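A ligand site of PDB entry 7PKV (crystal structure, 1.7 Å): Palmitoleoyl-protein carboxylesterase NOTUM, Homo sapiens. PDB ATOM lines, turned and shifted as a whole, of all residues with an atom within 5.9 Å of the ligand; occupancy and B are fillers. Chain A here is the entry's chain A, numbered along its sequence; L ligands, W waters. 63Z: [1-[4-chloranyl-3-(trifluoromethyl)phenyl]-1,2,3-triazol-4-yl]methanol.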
ATOM      1  N   GLY A  49      -2.778   3.446   2.217  1.00  0.00           N
ATOM      2  CA  GLY A  49      -2.415   2.627   3.344  1.00  0.00           C
ATOM      3  C   GLY A  49      -3.247   2.913   4.587  1.00  0.00           C
ATOM      4  O   GLY A  49      -4.317   3.521   4.523  1.00  0.00           O
ATOM      5  N   GLY A  50      -2.756   2.434   5.734  1.00  0.00           N
ATOM      6  CA  GLY A  50      -3.431   2.623   7.009  1.00  0.00           C
ATOM      7  C   GLY A  50      -3.595   1.364   7.847  1.00  0.00           C
ATOM      8  O   GLY A  50      -4.724   1.011   8.216  1.00  0.00           O
ATOM      9  N   TRP A  51      -2.483   0.690   8.177  1.00  0.00           N
ATOM     10  CA  TRP A  51      -2.475  -0.538   8.957  1.00  0.00           C
ATOM     11  C   TRP A  51      -3.423  -1.613   8.390  1.00  0.00           C
ATOM     12  O   TRP A  51      -3.438  -1.826   7.165  1.00  0.00           O
ATOM     13  CB  TRP A  51      -2.792  -0.220  10.418  1.00  0.00           C
ATOM     14  CG  TRP A  51      -1.714   0.614  11.064  1.00  0.00           C
ATOM     15  CD1 TRP A  51      -1.735   1.954  11.282  1.00  0.00           C
ATOM     16  CD2 TRP A  51      -0.430   0.147  11.519  1.00  0.00           C
ATOM     17  NE1 TRP A  51      -0.545   2.365  11.857  1.00  0.00           N
ATOM     18  CE2 TRP A  51       0.268   1.270  12.022  1.00  0.00           C
ATOM     19  CE3 TRP A  51       0.195  -1.105  11.561  1.00  0.00           C
ATOM     20  CZ2 TRP A  51       1.554   1.177  12.569  1.00  0.00           C
ATOM     21  CZ3 TRP A  51       1.474  -1.209  12.102  1.00  0.00           C
ATOM     22  CH2 TRP A  51       2.138  -0.069  12.604  1.00  0.00           C
ATOM     23  N   TYR A  52      -4.145  -2.306   9.263  1.00  0.00           N
ATOM     24  CA  TYR A  52      -4.868  -3.542   8.939  1.00  0.00           C
ATOM     25  C   TYR A  52      -5.592  -3.999  10.200  1.00  0.00           C
ATOM     26  O   TYR A  52      -5.400  -3.445  11.277  1.00  0.00           O
ATOM     27  CB  TYR A  52      -3.927  -4.649   8.429  1.00  0.00           C
ATOM     28  CG  TYR A  52      -2.659  -4.765   9.245  1.00  0.00           C
ATOM     29  CD1 TYR A  52      -2.645  -5.420  10.476  1.00  0.00           C
ATOM     30  CD2 TYR A  52      -1.470  -4.210   8.801  1.00  0.00           C
ATOM     31  CE1 TYR A  52      -1.484  -5.510  11.235  1.00  0.00           C
ATOM     32  CE2 TYR A  52      -0.304  -4.298   9.550  1.00  0.00           C
ATOM     33  CZ  TYR A  52      -0.324  -4.943  10.757  1.00  0.00           C
ATOM     34  OH  TYR A  52       0.856  -5.004  11.475  1.00  0.00           O
ATOM     35  N   VAL A 110      -3.845  -5.374   3.950  1.00  0.00           N
ATOM     36  CA  VAL A 110      -2.613  -5.096   3.219  1.00  0.00           C
ATOM     37  C   VAL A 110      -2.784  -5.442   1.734  1.00  0.00           C
ATOM     38  O   VAL A 110      -1.829  -5.818   1.048  1.00  0.00           O
ATOM     39  CB  VAL A 110      -1.402  -5.834   3.853  1.00  0.00           C
ATOM     40  CG1 VAL A 110      -0.116  -5.153   3.403  1.00  0.00           C
ATOM     41  CG2 VAL A 110      -1.501  -5.804   5.380  1.00  0.00           C
ATOM     42  N   SER A 155       2.618   2.951   2.807  1.00  0.00           N
ATOM     43  CA  SER A 155       2.322   2.216   4.043  1.00  0.00           C
ATOM     44  C   SER A 155       1.802   0.832   3.660  1.00  0.00           C
ATOM     45  O   SER A 155       2.467   0.114   2.899  1.00  0.00           O
ATOM     46  CB  SER A 155       1.401   3.069   4.903  1.00  0.00           C
ATOM     47  OG  SER A 155       0.562   2.259   5.708  1.00  0.00           O
ATOM     48  N   ALA A 156       0.634   0.403   4.163  1.00  0.00           N
ATOM     49  CA  ALA A 156       0.074  -0.878   3.737  1.00  0.00           C
ATOM     50  C   ALA A 156      -0.087  -0.922   2.219  1.00  0.00           C
ATOM     51  O   ALA A 156      -0.016  -1.994   1.619  1.00  0.00           O
ATOM     52  CB  ALA A 156      -1.274  -1.134   4.428  1.00  0.00           C
ATOM     53  N   THR A 159       3.318  -2.049   0.746  1.00  0.00           N
ATOM     54  CA  THR A 159       3.396  -3.504   0.790  1.00  0.00           C
ATOM     55  C   THR A 159       2.447  -4.090  -0.237  1.00  0.00           C
ATOM     56  O   THR A 159       2.783  -5.090  -0.888  1.00  0.00           O
ATOM     57  CB  THR A 159       3.079  -4.032   2.184  1.00  0.00           C
ATOM     58  OG1 THR A 159       3.885  -3.343   3.154  1.00  0.00           O
ATOM     59  CG2 THR A 159       3.419  -5.520   2.266  1.00  0.00           C
ATOM     60  N   SER A 188       7.253   3.261   1.898  1.00  0.00           N
ATOM     61  CA  SER A 188       7.019   3.004   3.322  1.00  0.00           C
ATOM     62  C   SER A 188       6.325   1.666   3.565  1.00  0.00           C
ATOM     63  O   SER A 188       5.536   1.533   4.514  1.00  0.00           O
ATOM     64  CB  SER A 188       6.214   4.140   3.959  1.00  0.00           C
ATOM     65  OG  SER A 188       6.953   5.342   3.912  1.00  0.00           O
ATOM     66  N   GLY A 189       6.634   0.668   2.743  1.00  0.00           N
ATOM     67  CA  GLY A 189       6.027  -0.646   2.897  1.00  0.00           C
ATOM     68  C   GLY A 189       7.052  -1.747   2.948  1.00  0.00           C
ATOM     69  O   GLY A 189       6.721  -2.910   2.678  1.00  0.00           O
ATOM     70  N   PHE A 191       9.351  -3.540   5.396  1.00  0.00           N
ATOM     71  CA  PHE A 191       9.491  -3.770   6.824  1.00  0.00           C
ATOM     72  C   PHE A 191      10.439  -4.926   7.108  1.00  0.00           C
ATOM     73  O   PHE A 191      10.694  -5.795   6.267  1.00  0.00           O
ATOM     74  CB  PHE A 191       8.118  -4.041   7.455  1.00  0.00           C
ATOM     75  CG  PHE A 191       7.196  -2.860   7.369  1.00  0.00           C
ATOM     76  CD1 PHE A 191       7.333  -1.815   8.254  1.00  0.00           C
ATOM     77  CD2 PHE A 191       6.234  -2.788   6.363  1.00  0.00           C
ATOM     78  CE1 PHE A 191       6.495  -0.694   8.161  1.00  0.00           C
ATOM     79  CE2 PHE A 191       5.405  -1.667   6.275  1.00  0.00           C
ATOM     80  CZ  PHE A 191       5.535  -0.636   7.176  1.00  0.00           C
ATOM     81  N   LEU A 192      10.955  -4.925   8.335  1.00  0.00           N
ATOM     82  CA  LEU A 192      11.861  -5.956   8.828  1.00  0.00           C
ATOM     83  C   LEU A 192      11.136  -6.806   9.859  1.00  0.00           C
ATOM     84  O   LEU A 192      10.473  -6.272  10.751  1.00  0.00           O
ATOM     85  CB  LEU A 192      13.100  -5.324   9.462  1.00  0.00           C
ATOM     86  CG  LEU A 192      13.912  -4.418   8.541  1.00  0.00           C
ATOM     87  CD1 LEU A 192      15.150  -3.911   9.260  1.00  0.00           C
ATOM     88  CD2 LEU A 192      14.286  -5.143   7.257  1.00  0.00           C
ATOM     89  N   PRO A 210       4.244  -8.685  14.841  1.00  0.00           N
ATOM     90  CA  PRO A 210       4.464  -8.348  13.416  1.00  0.00           C
ATOM     91  C   PRO A 210       4.397  -9.587  12.523  1.00  0.00           C
ATOM     92  O   PRO A 210       3.545  -9.664  11.650  1.00  0.00           O
ATOM     93  CB  PRO A 210       5.858  -7.722  13.412  1.00  0.00           C
ATOM     94  CG  PRO A 210       6.043  -7.204  14.782  1.00  0.00           C
ATOM     95  CD  PRO A 210       5.302  -8.140  15.697  1.00  0.00           C
ATOM     96  N   THR A 211       5.292 -10.548  12.755  1.00  0.00           N
ATOM     97  CA  THR A 211       5.141 -11.828  12.062  1.00  0.00           C
ATOM     98  C   THR A 211       3.862 -12.533  12.477  1.00  0.00           C
ATOM     99  O   THR A 211       3.180 -13.123  11.632  1.00  0.00           O
ATOM    100  CB  THR A 211       6.351 -12.714  12.325  1.00  0.00           C
ATOM    101  OG1 THR A 211       6.419 -13.010  13.727  1.00  0.00           O
ATOM    102  CG2 THR A 211       7.639 -12.018  11.913  1.00  0.00           C
ATOM    103  N   ALA A 213       1.057 -11.134  13.672  1.00  0.00           N
ATOM    104  CA  ALA A 213      -0.053 -10.373  13.103  1.00  0.00           C
ATOM    105  C   ALA A 213      -0.359 -10.796  11.672  1.00  0.00           C
ATOM    106  O   ALA A 213      -1.497 -11.115  11.345  1.00  0.00           O
ATOM    107  CB  ALA A 213       0.269  -8.874  13.169  1.00  0.00           C
ATOM    108  N   ILE A 214       0.678 -10.831  10.827  1.00  0.00           N
ATOM    109  CA  ILE A 214       0.501 -11.232   9.429  1.00  0.00           C
ATOM    110  C   ILE A 214       0.074 -12.697   9.320  1.00  0.00           C
ATOM    111  O   ILE A 214      -0.777 -13.058   8.500  1.00  0.00           O
ATOM    112  CB  ILE A 214       1.795 -10.948   8.639  1.00  0.00           C
ATOM    113  CG1 ILE A 214       2.232  -9.467   8.722  1.00  0.00           C
ATOM    114  CG2 ILE A 214       1.645 -11.357   7.184  1.00  0.00           C
ATOM    115  CD1 ILE A 214       1.205  -8.466   8.322  1.00  0.00           C
ATOM    116  N   PHE A 242       5.111 -10.968   2.837  1.00  0.00           N
ATOM    117  CA  PHE A 242       4.748  -9.599   3.182  1.00  0.00           C
ATOM    118  C   PHE A 242       5.959  -8.757   3.553  1.00  0.00           C
ATOM    119  O   PHE A 242       5.806  -7.548   3.783  1.00  0.00           O
ATOM    120  CB  PHE A 242       3.767  -9.558   4.370  1.00  0.00           C
ATOM    121  CG  PHE A 242       2.365  -9.927   4.019  1.00  0.00           C
ATOM    122  CD1 PHE A 242       2.083 -11.200   3.569  1.00  0.00           C
ATOM    123  CD2 PHE A 242       1.313  -9.029   4.206  1.00  0.00           C
ATOM    124  CE1 PHE A 242       0.794 -11.571   3.261  1.00  0.00           C
ATOM    125  CE2 PHE A 242       0.006  -9.402   3.888  1.00  0.00           C
ATOM    126  CZ  PHE A 242      -0.245 -10.667   3.421  1.00  0.00           C
ATOM    127  N   PHE A 243       7.141  -9.354   3.639  1.00  0.00           N
ATOM    128  CA  PHE A 243       8.342  -8.614   3.996  1.00  0.00           C
ATOM    129  C   PHE A 243       9.148  -8.341   2.745  1.00  0.00           C
ATOM    130  O   PHE A 243       9.610  -9.272   2.080  1.00  0.00           O
ATOM    131  CB  PHE A 243       9.113  -9.380   5.056  1.00  0.00           C
ATOM    132  CG  PHE A 243       8.421  -9.340   6.359  1.00  0.00           C
ATOM    133  CD1 PHE A 243       8.642  -8.283   7.231  1.00  0.00           C
ATOM    134  CD2 PHE A 243       7.435 -10.255   6.654  1.00  0.00           C
ATOM    135  CE1 PHE A 243       7.950  -8.183   8.411  1.00  0.00           C
ATOM    136  CE2 PHE A 243       6.732 -10.177   7.836  1.00  0.00           C
ATOM    137  CZ  PHE A 243       6.991  -9.128   8.724  1.00  0.00           C
ATOM    138  N   ALA A 265       6.508   3.513  11.610  1.00  0.00           N
ATOM    139  CA  ALA A 265       5.693   2.311  11.790  1.00  0.00           C
ATOM    140  C   ALA A 265       6.552   1.112  12.147  1.00  0.00           C
ATOM    141  O   ALA A 265       6.130   0.247  12.924  1.00  0.00           O
ATOM    142  CB  ALA A 265       4.864   2.038  10.549  1.00  0.00           C
ATOM    143  N   GLN A 266       7.759   1.026  11.575  1.00  0.00           N
ATOM    144  CA  GLN A 266       8.692  -0.012  12.013  1.00  0.00           C
ATOM    145  C   GLN A 266       9.032   0.142  13.493  1.00  0.00           C
ATOM    146  O   GLN A 266       9.049  -0.838  14.251  1.00  0.00           O
ATOM    147  CB  GLN A 266       9.960   0.047  11.140  1.00  0.00           C
ATOM    148  CG  GLN A 266      11.009  -0.979  11.522  1.00  0.00           C
ATOM    149  CD  GLN A 266      10.714  -2.360  10.975  1.00  0.00           C
ATOM    150  OE1 GLN A 266      10.460  -2.547   9.778  1.00  0.00           O
ATOM    151  NE2 GLN A 266      10.789  -3.370  11.845  1.00  0.00           N
ATOM    152  N   VAL A 269       6.019  -1.093  15.676  1.00  0.00           N
ATOM    153  CA  VAL A 269       5.907  -2.538  15.834  1.00  0.00           C
ATOM    154  C   VAL A 269       7.114  -3.099  16.571  1.00  0.00           C
ATOM    155  O   VAL A 269       7.040  -4.218  17.098  1.00  0.00           O
ATOM    156  CB  VAL A 269       5.678  -3.239  14.482  1.00  0.00           C
ATOM    157  CG1 VAL A 269       4.389  -2.742  13.828  1.00  0.00           C
ATOM    158  CG2 VAL A 269       6.873  -3.066  13.543  1.00  0.00           C
ATOM    159  N   HIS A 312       7.144   8.975   8.406  1.00  0.00           N
ATOM    160  CA  HIS A 312       6.141   7.983   7.989  1.00  0.00           C
ATOM    161  C   HIS A 312       5.487   8.425   6.678  1.00  0.00           C
ATOM    162  O   HIS A 312       4.802   9.441   6.670  1.00  0.00           O
ATOM    163  CB  HIS A 312       5.083   7.804   9.083  1.00  0.00           C
ATOM    164  CG  HIS A 312       3.997   6.834   8.721  1.00  0.00           C
ATOM    165  ND1 HIS A 312       4.263   5.547   8.292  1.00  0.00           N
ATOM    166  CD2 HIS A 312       2.653   6.948   8.726  1.00  0.00           C
ATOM    167  CE1 HIS A 312       3.134   4.920   8.050  1.00  0.00           C
ATOM    168  NE2 HIS A 312       2.131   5.754   8.302  1.00  0.00           N
ATOM    169  N   GLU A 313       5.690   7.634   5.614  1.00  0.00           N
ATOM    170  CA  GLU A 313       5.175   7.869   4.246  1.00  0.00           C
ATOM    171  C   GLU A 313       5.842   9.073   3.591  1.00  0.00           C
ATOM    172  O   GLU A 313       6.542   9.834   4.266  1.00  0.00           O
ATOM    173  CB  GLU A 313       3.660   8.077   4.224  1.00  0.00           C
ATOM    174  CG  GLU A 313       2.857   6.907   4.743  1.00  0.00           C
ATOM    175  CD  GLU A 313       1.361   7.142   4.702  1.00  0.00           C
ATOM    176  OE1 GLU A 313       0.945   8.323   4.766  1.00  0.00           O
ATOM    177  OE2 GLU A 313       0.586   6.149   4.618  1.00  0.00           O
HETATM  178  N1  63Z L   1       0.816  -1.207   7.324  1.00  0.00           N
HETATM  179  C2  63Z L   1       4.640  -5.225   9.788  1.00  0.00           C
HETATM  180  C4  63Z L   1       2.587  -2.766   7.790  1.00  0.00           C
HETATM  181  C5  63Z L   1       1.463   0.551   8.434  1.00  0.00           C
HETATM  182  C6  63Z L   1       1.385   1.962   8.945  1.00  0.00           C
HETATM  183  C8  63Z L   1       2.553  -3.363   6.530  1.00  0.00           C
HETATM  184  C9  63Z L   1       3.218  -4.552   6.323  1.00  0.00           C
HETATM  185  N   63Z L   1       1.962  -1.497   7.976  1.00  0.00           N
HETATM  186  C   63Z L   1       3.900  -5.154   7.366  1.00  0.00           C
HETATM  187  O   63Z L   1       0.331   2.665   8.334  1.00  0.00           O
HETATM  188  C1  63Z L   1       3.929  -4.580   8.640  1.00  0.00           C
HETATM  189  C3  63Z L   1       3.265  -3.370   8.841  1.00  0.00           C
HETATM  190  C7  63Z L   1       2.384  -0.430   8.686  1.00  0.00           C
HETATM  191  F   63Z L   1       5.927  -5.429   9.523  1.00  0.00           F
HETATM  192  F1  63Z L   1       4.577  -4.507  10.915  1.00  0.00           F
HETATM  193  F2  63Z L   1       4.138  -6.435  10.082  1.00  0.00           F
HETATM  194  N2  63Z L   1       0.526   0.049   7.600  1.00  0.00           N
HETATM  195 CL   63Z L   1       4.758  -6.624   7.021  1.00  0.00          CL
HETATM  196  O   HOH W   1      -0.593   4.947   8.245  1.00  0.00           O
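The side-chain hydroxyl (OG) of Ser 155 sits at hydrogen-bond distance from an oxygen (O) of the ligand. The backbone NH of Trp 51 is in hydrogen-bond range of a nitrogen (N2) of the ligand (3.1 Å). A nitrogen (N2) of the ligand lies within hydrogen-bond range of the backbone NH (N) of Ala 156, 3.5 Å away.
OG of Ser 155 sits at hydrogen-bond distance from N of Gly 50 (3.3 Å). The side-chain hydroxyl of Thr 159 is in hydrogen-bond range of the backbone carbonyl oxygen of Gly 189 (2.9 Å).
Merely in contact with the ligand: Gly 50 (3.99 Å), Tyr 52 (3.7 Å), Thr 159 (3.5 Å), Phe 191 (3.3 Å), Pro 210 (3.6 Å), Ile 214 (3.8 Å), Phe 242 (3.5 Å), Phe 243 (3.6 Å), Ala 265 (3.8 Å), Val 269 (3.4 Å) and His 312 (3.6 Å). Hydrophobic or aromatic side chains within 4 Å of the ligand: Trp 51, Tyr 52, Ala 156, Phe 191, Pro 210, Ile 214, Phe 243, Ala 265, Val 269 and His 312. 14 residues have an atom within 4 Å of the ligand: Gly 50, Trp 51, Tyr 52, Ser 155, Ala 156, Thr 159, Phe 191, Pro 210, Ile 214, Phe 242, Phe 243, Ala 265, Val 269 and His 312.
Water W1 bridges O of the ligand (2.5 Å) and NE2 of His 312 (2.8 Å).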
